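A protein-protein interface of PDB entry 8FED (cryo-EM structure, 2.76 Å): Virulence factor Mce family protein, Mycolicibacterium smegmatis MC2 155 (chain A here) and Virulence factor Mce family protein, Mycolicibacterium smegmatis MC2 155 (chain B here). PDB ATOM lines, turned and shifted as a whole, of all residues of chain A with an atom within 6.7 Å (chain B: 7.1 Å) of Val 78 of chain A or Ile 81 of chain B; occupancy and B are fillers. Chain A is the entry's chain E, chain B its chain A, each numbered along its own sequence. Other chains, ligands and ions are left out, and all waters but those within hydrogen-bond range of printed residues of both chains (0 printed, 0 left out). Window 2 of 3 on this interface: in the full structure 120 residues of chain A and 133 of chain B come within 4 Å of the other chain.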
ATOM      1  N   VAL A  73      -3.796 -17.288 -18.069  1.00  0.00           N
ATOM      2  CA  VAL A  73      -3.618 -16.753 -19.412  1.00  0.00           C
ATOM      3  C   VAL A  73      -2.240 -17.178 -19.893  1.00  0.00           C
ATOM      4  O   VAL A  73      -1.227 -16.865 -19.256  1.00  0.00           O
ATOM      5  CB  VAL A  73      -3.774 -15.225 -19.433  1.00  0.00           C
ATOM      6  CG1 VAL A  73      -3.412 -14.673 -20.799  1.00  0.00           C
ATOM      7  CG2 VAL A  73      -5.192 -14.850 -19.062  1.00  0.00           C
ATOM      8  N   ARG A  74      -2.203 -17.890 -21.014  1.00  0.00           N
ATOM      9  CA  ARG A  74      -0.999 -18.540 -21.501  1.00  0.00           C
ATOM     10  C   ARG A  74      -0.598 -17.964 -22.851  1.00  0.00           C
ATOM     11  O   ARG A  74      -1.419 -17.888 -23.773  1.00  0.00           O
ATOM     12  CB  ARG A  74      -1.202 -20.052 -21.609  1.00  0.00           C
ATOM     13  CG  ARG A  74      -1.460 -20.730 -20.276  1.00  0.00           C
ATOM     14  CD  ARG A  74      -1.509 -22.236 -20.421  1.00  0.00           C
ATOM     15  NE  ARG A  74      -1.708 -22.903 -19.141  1.00  0.00           N
ATOM     16  CZ  ARG A  74      -0.730 -23.241 -18.312  1.00  0.00           C
ATOM     17  NH1 ARG A  74       0.535 -22.976 -18.591  1.00  0.00           N
ATOM     18  NH2 ARG A  74      -1.028 -23.863 -17.177  1.00  0.00           N
ATOM     19  N   VAL A  75       0.662 -17.561 -22.952  1.00  0.00           N
ATOM     20  CA  VAL A  75       1.295 -17.215 -24.218  1.00  0.00           C
ATOM     21  C   VAL A  75       2.386 -18.242 -24.476  1.00  0.00           C
ATOM     22  O   VAL A  75       3.251 -18.460 -23.618  1.00  0.00           O
ATOM     23  CB  VAL A  75       1.868 -15.788 -24.201  1.00  0.00           C
ATOM     24  CG1 VAL A  75       2.541 -15.472 -25.526  1.00  0.00           C
ATOM     25  CG2 VAL A  75       0.768 -14.781 -23.909  1.00  0.00           C
ATOM     26  N   ARG A  76       2.331 -18.885 -25.646  1.00  0.00           N
ATOM     27  CA  ARG A  76       3.226 -19.992 -25.992  1.00  0.00           C
ATOM     28  C   ARG A  76       3.154 -21.100 -24.943  1.00  0.00           C
ATOM     29  O   ARG A  76       4.168 -21.691 -24.569  1.00  0.00           O
ATOM     30  CB  ARG A  76       4.666 -19.510 -26.182  1.00  0.00           C
ATOM     31  CG  ARG A  76       4.865 -18.639 -27.408  1.00  0.00           C
ATOM     32  CD  ARG A  76       4.656 -19.435 -28.680  1.00  0.00           C
ATOM     33  NE  ARG A  76       4.860 -18.627 -29.876  1.00  0.00           N
ATOM     34  CZ  ARG A  76       3.892 -18.248 -30.698  1.00  0.00           C
ATOM     35  NH1 ARG A  76       2.634 -18.599 -30.491  1.00  0.00           N
ATOM     36  NH2 ARG A  76       4.195 -17.505 -31.758  1.00  0.00           N
ATOM     37  N   ASP A  77       1.938 -21.365 -24.460  1.00  0.00           N
ATOM     38  CA  ASP A  77       1.652 -22.340 -23.407  1.00  0.00           C
ATOM     39  C   ASP A  77       2.377 -22.023 -22.104  1.00  0.00           C
ATOM     40  O   ASP A  77       2.594 -22.915 -21.279  1.00  0.00           O
ATOM     41  CB  ASP A  77       1.972 -23.770 -23.859  1.00  0.00           C
ATOM     42  CG  ASP A  77       1.019 -24.269 -24.924  1.00  0.00           C
ATOM     43  OD1 ASP A  77       0.106 -23.509 -25.309  1.00  0.00           O
ATOM     44  OD2 ASP A  77       1.177 -25.422 -25.373  1.00  0.00           O
ATOM     45  N   VAL A  78       2.745 -20.762 -21.894  1.00  0.00           N
ATOM     46  CA  VAL A  78       3.403 -20.315 -20.673  1.00  0.00           C
ATOM     47  C   VAL A  78       2.436 -19.420 -19.914  1.00  0.00           C
ATOM     48  O   VAL A  78       1.914 -18.447 -20.473  1.00  0.00           O
ATOM     49  CB  VAL A  78       4.715 -19.574 -20.971  1.00  0.00           C
ATOM     50  CG1 VAL A  78       5.368 -19.116 -19.680  1.00  0.00           C
ATOM     51  CG2 VAL A  78       5.657 -20.455 -21.764  1.00  0.00           C
ATOM     52  N   PHE A  79       2.192 -19.757 -18.649  1.00  0.00           N
ATOM     53  CA  PHE A  79       1.281 -19.004 -17.794  1.00  0.00           C
ATOM     54  C   PHE A  79       1.913 -17.664 -17.437  1.00  0.00           C
ATOM     55  O   PHE A  79       2.871 -17.605 -16.662  1.00  0.00           O
ATOM     56  CB  PHE A  79       0.960 -19.832 -16.552  1.00  0.00           C
ATOM     57  CG  PHE A  79       0.563 -19.023 -15.350  1.00  0.00           C
ATOM     58  CD1 PHE A  79      -0.636 -18.337 -15.318  1.00  0.00           C
ATOM     59  CD2 PHE A  79       1.380 -18.981 -14.235  1.00  0.00           C
ATOM     60  CE1 PHE A  79      -1.003 -17.609 -14.204  1.00  0.00           C
ATOM     61  CE2 PHE A  79       1.018 -18.255 -13.123  1.00  0.00           C
ATOM     62  CZ  PHE A  79      -0.176 -17.567 -13.107  1.00  0.00           C
ATOM     63  N   VAL A  80       1.395 -16.585 -18.026  1.00  0.00           N
ATOM     64  CA  VAL A  80       1.987 -15.262 -17.860  1.00  0.00           C
ATOM     65  C   VAL A  80       0.923 -14.230 -17.514  1.00  0.00           C
ATOM     66  O   VAL A  80       1.180 -13.022 -17.569  1.00  0.00           O
ATOM     67  CB  VAL A  80       2.751 -14.843 -19.128  1.00  0.00           C
ATOM     68  CG1 VAL A  80       4.063 -15.602 -19.240  1.00  0.00           C
ATOM     69  CG2 VAL A  80       1.892 -15.079 -20.355  1.00  0.00           C
ATOM     70  N   GLY A  81      -0.274 -14.683 -17.160  1.00  0.00           N
ATOM     71  CA  GLY A  81      -1.341 -13.740 -16.882  1.00  0.00           C
ATOM     72  C   GLY A  81      -2.514 -14.415 -16.209  1.00  0.00           C
ATOM     73  O   GLY A  81      -2.534 -15.632 -16.010  1.00  0.00           O
ATOM     74  N   GLY B  56       9.766 -23.778 -29.021  1.00  0.00           N
ATOM     75  CA  GLY B  56       8.678 -23.000 -29.590  1.00  0.00           C
ATOM     76  C   GLY B  56       7.562 -22.753 -28.593  1.00  0.00           C
ATOM     77  O   GLY B  56       7.024 -21.647 -28.510  1.00  0.00           O
ATOM     78  N   ARG B  57       7.202 -23.777 -27.824  1.00  0.00           N
ATOM     79  CA  ARG B  57       6.196 -23.642 -26.785  1.00  0.00           C
ATOM     80  C   ARG B  57       6.565 -24.549 -25.622  1.00  0.00           C
ATOM     81  O   ARG B  57       7.211 -25.583 -25.804  1.00  0.00           O
ATOM     82  CB  ARG B  57       4.794 -23.979 -27.305  1.00  0.00           C
ATOM     83  CG  ARG B  57       4.626 -25.403 -27.799  1.00  0.00           C
ATOM     84  CD  ARG B  57       3.209 -25.638 -28.284  1.00  0.00           C
ATOM     85  NE  ARG B  57       2.998 -27.006 -28.737  1.00  0.00           N
ATOM     86  CZ  ARG B  57       2.535 -27.983 -27.970  1.00  0.00           C
ATOM     87  NH1 ARG B  57       2.241 -27.780 -26.698  1.00  0.00           N
ATOM     88  NH2 ARG B  57       2.364 -29.193 -28.494  1.00  0.00           N
ATOM     89  N   ALA B  58       6.153 -24.146 -24.418  1.00  0.00           N
ATOM     90  CA  ALA B  58       6.507 -24.904 -23.225  1.00  0.00           C
ATOM     91  C   ALA B  58       5.724 -26.204 -23.125  1.00  0.00           C
ATOM     92  O   ALA B  58       6.237 -27.195 -22.595  1.00  0.00           O
ATOM     93  CB  ALA B  58       6.281 -24.055 -21.976  1.00  0.00           C
ATOM     94  N   GLY B  59       4.490 -26.225 -23.617  1.00  0.00           N
ATOM     95  CA  GLY B  59       3.655 -27.401 -23.492  1.00  0.00           C
ATOM     96  C   GLY B  59       2.785 -27.349 -22.255  1.00  0.00           C
ATOM     97  O   GLY B  59       3.244 -26.945 -21.183  1.00  0.00           O
ATOM     98  N   LEU B  60       1.523 -27.746 -22.391  1.00  0.00           N
ATOM     99  CA  LEU B  60       0.604 -27.714 -21.265  1.00  0.00           C
ATOM    100  C   LEU B  60       0.975 -28.786 -20.246  1.00  0.00           C
ATOM    101  O   LEU B  60       1.668 -29.758 -20.555  1.00  0.00           O
ATOM    102  CB  LEU B  60      -0.834 -27.917 -21.739  1.00  0.00           C
ATOM    103  CG  LEU B  60      -1.358 -26.912 -22.764  1.00  0.00           C
ATOM    104  CD1 LEU B  60      -2.793 -27.234 -23.131  1.00  0.00           C
ATOM    105  CD2 LEU B  60      -1.241 -25.495 -22.237  1.00  0.00           C
ATOM    106  N   MET B  62       3.049 -28.529 -17.953  1.00  0.00           N
ATOM    107  CA  MET B  62       4.474 -28.442 -17.649  1.00  0.00           C
ATOM    108  C   MET B  62       4.673 -27.218 -16.763  1.00  0.00           C
ATOM    109  O   MET B  62       4.704 -26.082 -17.248  1.00  0.00           O
ATOM    110  CB  MET B  62       5.317 -28.367 -18.919  1.00  0.00           C
ATOM    111  CG  MET B  62       6.779 -28.021 -18.670  1.00  0.00           C
ATOM    112  SD  MET B  62       7.875 -28.521 -20.006  1.00  0.00           S
ATOM    113  CE  MET B  62       7.791 -30.300 -19.858  1.00  0.00           C
ATOM    114  N   ASP B  63       4.785 -27.457 -15.464  1.00  0.00           N
ATOM    115  CA  ASP B  63       4.971 -26.442 -14.443  1.00  0.00           C
ATOM    116  C   ASP B  63       6.299 -26.688 -13.740  1.00  0.00           C
ATOM    117  O   ASP B  63       6.879 -27.771 -13.871  1.00  0.00           O
ATOM    118  CB  ASP B  63       3.817 -26.484 -13.430  1.00  0.00           C
ATOM    119  CG  ASP B  63       2.478 -26.137 -14.054  1.00  0.00           C
ATOM    120  OD1 ASP B  63       2.424 -25.189 -14.865  1.00  0.00           O
ATOM    121  OD2 ASP B  63       1.478 -26.813 -13.734  1.00  0.00           O
ATOM    122  N   PRO B  64       6.834 -25.692 -13.027  1.00  0.00           N
ATOM    123  CA  PRO B  64       8.072 -25.916 -12.270  1.00  0.00           C
ATOM    124  C   PRO B  64       7.939 -27.094 -11.315  1.00  0.00           C
ATOM    125  O   PRO B  64       6.906 -27.287 -10.672  1.00  0.00           O
ATOM    126  CB  PRO B  64       8.266 -24.596 -11.522  1.00  0.00           C
ATOM    127  CG  PRO B  64       7.647 -23.588 -12.411  1.00  0.00           C
ATOM    128  CD  PRO B  64       6.461 -24.266 -13.044  1.00  0.00           C
ATOM    129  N   SER B  66       8.780 -30.212 -12.712  1.00  0.00           N
ATOM    130  CA  SER B  66       8.661 -31.345 -13.618  1.00  0.00           C
ATOM    131  C   SER B  66      10.001 -32.052 -13.759  1.00  0.00           C
ATOM    132  O   SER B  66      11.055 -31.413 -13.814  1.00  0.00           O
ATOM    133  CB  SER B  66       8.162 -30.889 -14.988  1.00  0.00           C
ATOM    134  OG  SER B  66       6.815 -30.459 -14.923  1.00  0.00           O
ATOM    135  N   LEU B  78      12.632 -29.223 -13.211  1.00  0.00           N
ATOM    136  CA  LEU B  78      12.443 -27.950 -13.889  1.00  0.00           C
ATOM    137  C   LEU B  78      12.333 -26.826 -12.870  1.00  0.00           C
ATOM    138  O   LEU B  78      11.539 -26.902 -11.929  1.00  0.00           O
ATOM    139  CB  LEU B  78      11.185 -28.006 -14.755  1.00  0.00           C
ATOM    140  CG  LEU B  78      10.646 -26.734 -15.415  1.00  0.00           C
ATOM    141  CD1 LEU B  78      11.642 -26.099 -16.355  1.00  0.00           C
ATOM    142  CD2 LEU B  78       9.357 -27.058 -16.148  1.00  0.00           C
ATOM    143  N   ALA B  79      13.132 -25.780 -13.065  1.00  0.00           N
ATOM    144  CA  ALA B  79      13.180 -24.671 -12.121  1.00  0.00           C
ATOM    145  C   ALA B  79      12.207 -23.568 -12.523  1.00  0.00           C
ATOM    146  O   ALA B  79      11.347 -23.174 -11.730  1.00  0.00           O
ATOM    147  CB  ALA B  79      14.605 -24.124 -12.001  1.00  0.00           C
ATOM    148  N   SER B  80      12.330 -23.057 -13.748  1.00  0.00           N
ATOM    149  CA  SER B  80      11.466 -21.943 -14.127  1.00  0.00           C
ATOM    150  C   SER B  80      11.159 -21.964 -15.617  1.00  0.00           C
ATOM    151  O   SER B  80      11.887 -22.554 -16.414  1.00  0.00           O
ATOM    152  CB  SER B  80      12.086 -20.593 -13.745  1.00  0.00           C
ATOM    153  OG  SER B  80      12.234 -20.475 -12.341  1.00  0.00           O
ATOM    154  N   ILE B  81      10.051 -21.314 -15.978  1.00  0.00           N
ATOM    155  CA  ILE B  81       9.633 -21.140 -17.366  1.00  0.00           C
ATOM    156  C   ILE B  81       9.357 -19.661 -17.604  1.00  0.00           C
ATOM    157  O   ILE B  81       8.730 -18.997 -16.772  1.00  0.00           O
ATOM    158  CB  ILE B  81       8.379 -21.977 -17.700  1.00  0.00           C
ATOM    159  CG1 ILE B  81       8.579 -23.439 -17.309  1.00  0.00           C
ATOM    160  CG2 ILE B  81       8.050 -21.880 -19.179  1.00  0.00           C
ATOM    161  CD1 ILE B  81       7.403 -24.314 -17.658  1.00  0.00           C
ATOM    162  N   ASP B  82       9.821 -19.146 -18.742  1.00  0.00           N
ATOM    163  CA  ASP B  82       9.639 -17.742 -19.080  1.00  0.00           C
ATOM    164  C   ASP B  82       9.384 -17.619 -20.576  1.00  0.00           C
ATOM    165  O   ASP B  82       9.628 -18.551 -21.344  1.00  0.00           O
ATOM    166  CB  ASP B  82      10.858 -16.906 -18.667  1.00  0.00           C
ATOM    167  CG  ASP B  82      10.526 -15.438 -18.476  1.00  0.00           C
ATOM    168  OD1 ASP B  82       9.620 -14.929 -19.170  1.00  0.00           O
ATOM    169  OD2 ASP B  82      11.173 -14.790 -17.627  1.00  0.00           O
ATOM    170  N   VAL B  83       8.875 -16.459 -20.984  1.00  0.00           N
ATOM    171  CA  VAL B  83       8.650 -16.139 -22.391  1.00  0.00           C
ATOM    172  C   VAL B  83       9.698 -15.122 -22.823  1.00  0.00           C
ATOM    173  O   VAL B  83       9.831 -14.058 -22.208  1.00  0.00           O
ATOM    174  CB  VAL B  83       7.233 -15.602 -22.637  1.00  0.00           C
ATOM    175  CG1 VAL B  83       7.138 -14.958 -24.009  1.00  0.00           C
ATOM    176  CG2 VAL B  83       6.224 -16.718 -22.525  1.00  0.00           C
ATOM    177  N   GLU B  91       9.105 -17.192 -27.550  1.00  0.00           N
ATOM    178  CA  GLU B  91       9.563 -18.561 -27.374  1.00  0.00           C
ATOM    179  C   GLU B  91       9.587 -18.877 -25.887  1.00  0.00           C
ATOM    180  O   GLU B  91       9.619 -17.976 -25.045  1.00  0.00           O
ATOM    181  CB  GLU B  91      10.956 -18.777 -27.982  1.00  0.00           C
ATOM    182  CG  GLU B  91      11.053 -18.440 -29.458  1.00  0.00           C
ATOM    183  CD  GLU B  91      12.470 -18.532 -29.982  1.00  0.00           C
ATOM    184  OE1 GLU B  91      13.395 -18.724 -29.165  1.00  0.00           O
ATOM    185  OE2 GLU B  91      12.659 -18.414 -31.211  1.00  0.00           O
ATOM    186  N   ALA B  92       9.566 -20.166 -25.561  1.00  0.00           N
ATOM    187  CA  ALA B  92       9.543 -20.608 -24.174  1.00  0.00           C
ATOM    188  C   ALA B  92      10.955 -20.989 -23.751  1.00  0.00           C
ATOM    189  O   ALA B  92      11.595 -21.829 -24.394  1.00  0.00           O
ATOM    190  CB  ALA B  92       8.589 -21.787 -23.992  1.00  0.00           C
ATOM    191  N   ARG B  93      11.434 -20.370 -22.677  1.00  0.00           N
ATOM    192  CA  ARG B  93      12.759 -20.627 -22.129  1.00  0.00           C
ATOM    193  C   ARG B  93      12.606 -21.295 -20.772  1.00  0.00           C
ATOM    194  O   ARG B  93      11.967 -20.741 -19.872  1.00  0.00           O
ATOM    195  CB  ARG B  93      13.560 -19.335 -21.994  1.00  0.00           C
ATOM    196  CG  ARG B  93      14.897 -19.519 -21.309  1.00  0.00           C
ATOM    197  CD  ARG B  93      15.671 -18.218 -21.234  1.00  0.00           C
ATOM    198  NE  ARG B  93      14.934 -17.186 -20.516  1.00  0.00           N
ATOM    199  CZ  ARG B  93      14.978 -17.012 -19.202  1.00  0.00           C
ATOM    200  NH1 ARG B  93      15.714 -17.791 -18.426  1.00  0.00           N
ATOM    201  NH2 ARG B  93      14.265 -16.033 -18.654  1.00  0.00           N
ATOM    202  N   LEU B  94      13.195 -22.474 -20.628  1.00  0.00           N
ATOM    203  CA  LEU B  94      13.094 -23.265 -19.413  1.00  0.00           C
ATOM    204  C   LEU B  94      14.460 -23.334 -18.747  1.00  0.00           C
ATOM    205  O   LEU B  94      15.454 -23.685 -19.392  1.00  0.00           O
ATOM    206  CB  LEU B  94      12.593 -24.681 -19.717  1.00  0.00           C
ATOM    207  CG  LEU B  94      11.181 -24.948 -20.253  1.00  0.00           C
ATOM    208  CD1 LEU B  94      11.005 -24.529 -21.705  1.00  0.00           C
ATOM    209  CD2 LEU B  94      10.843 -26.419 -20.092  1.00  0.00           C
ATOM    210  N   THR B  95      14.509 -23.002 -17.464  1.00  0.00           N
ATOM    211  CA  THR B  95      15.719 -23.139 -16.670  1.00  0.00           C
ATOM    212  C   THR B  95      15.580 -24.422 -15.867  1.00  0.00           C
ATOM    213  O   THR B  95      14.609 -24.579 -15.111  1.00  0.00           O
ATOM    214  CB  THR B  95      15.937 -21.938 -15.754  1.00  0.00           C
ATOM    215  OG1 THR B  95      14.801 -21.780 -14.899  1.00  0.00           O
ATOM    216  CG2 THR B  95      16.126 -20.674 -16.575  1.00  0.00           C
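The guanidinium group of Arg 57 of chain B is in salt-bridge range of the side-chain carboxylate of Asp 77 of chain A, at 2.9 Å.
The backbone NH of Ala 58 of chain B is in hydrogen-bond range of the backbone carbonyl oxygen of Arg 76 of chain A, 3.2 Å away.
NH1 of Arg 74 of chain A lies within hydrogen-bond range of O of Asp 77 of chain A, at 3.4 Å.
CD2 of Leu 60 of chain B touches CD of Arg 74 of chain A, at 3.7 Å.
Val 75 of chain A touches Val 83 of chain B.
Arg 76 of chain A touches Gly 56 of chain B (CD to O, 3.2 Å).
Arg 76 of chain A touches Arg 57 of chain B.
CB of Asp 77 of chain A touches N of Gly 59 of chain B, 3.5 Å away.
CD2 of Leu 60 of chain B touches CG of Asp 77 of chain A, 3.7 Å away.
Ala 58 of chain B touches Val 78 of chain A (CB to CG2, 3.7 Å).
CG2 of Ile 81 of chain B touches CG2 of Val 78 of chain A, at 3.8 Å.
CG2 of Val 83 of chain B touches CB of Val 78 of chain A, at 3.6 Å.
Val 78 of chain A touches Ala 92 of chain B (CG2 to CB, 3.9 Å).
Of the printed residues of chain B, Arg 76 of chain A touches Gly 56 (3.2 Å), Arg 57 (3.6 Å) and Ala 58 (3.2 Å).
Of the printed residues of chain A, Gly 56 of chain B touches Arg 76 (3.2 Å).
Of the printed residues of chain A, Arg 57 of chain B touches Arg 76 and Asp 77.
Asp 63 of chain B touches none of the printed residues of chain A.
Of chain A, only Val 78 (3.8 Å) comes within 4 Å of Ile 81 of chain B.
Printed residues of chain A within 4 Å of Val 83 of chain B: Val 75 and Val 78.
Of the printed residues of chain A, Ala 92 of chain B touches Val 78 (3.9 Å).
The nearest residue of chain B that does not touch Val 78 of chain A is Asp 82 of chain B (4.4 Å).
The nearest residue of chain A that does not touch Ile 81 of chain B is Asp 77 of chain A (5.9 Å).
Of the 9 printed residues of chain A, 5 touch a printed residue of chain B.
Printed residues of chain A that touch a printed residue of chain B: Arg 74, Val 75, Arg 76, Asp 77 and Val 78.
Hydrophobic or aromatic side chains of chain A within 4 Å of the printed part of chain B: Val 78.
Printed residues of chain B that touch a printed residue of chain A: Gly 56, Arg 57, Ala 58, Gly 59, Leu 60, Ile 81, Val 83 and Ala 92.
Hydrophobic or aromatic side chains of chain B within 4 Å of the printed part of chain A: Ala 58, Leu 60, Ile 81, Val 83 and Ala 92.
Among the printed residues, Asp or Glu carboxylates within 4 Å of a Lys or Arg side-chain nitrogen of the other chain: Asp 77 of chain A with Arg 57 of chain B.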
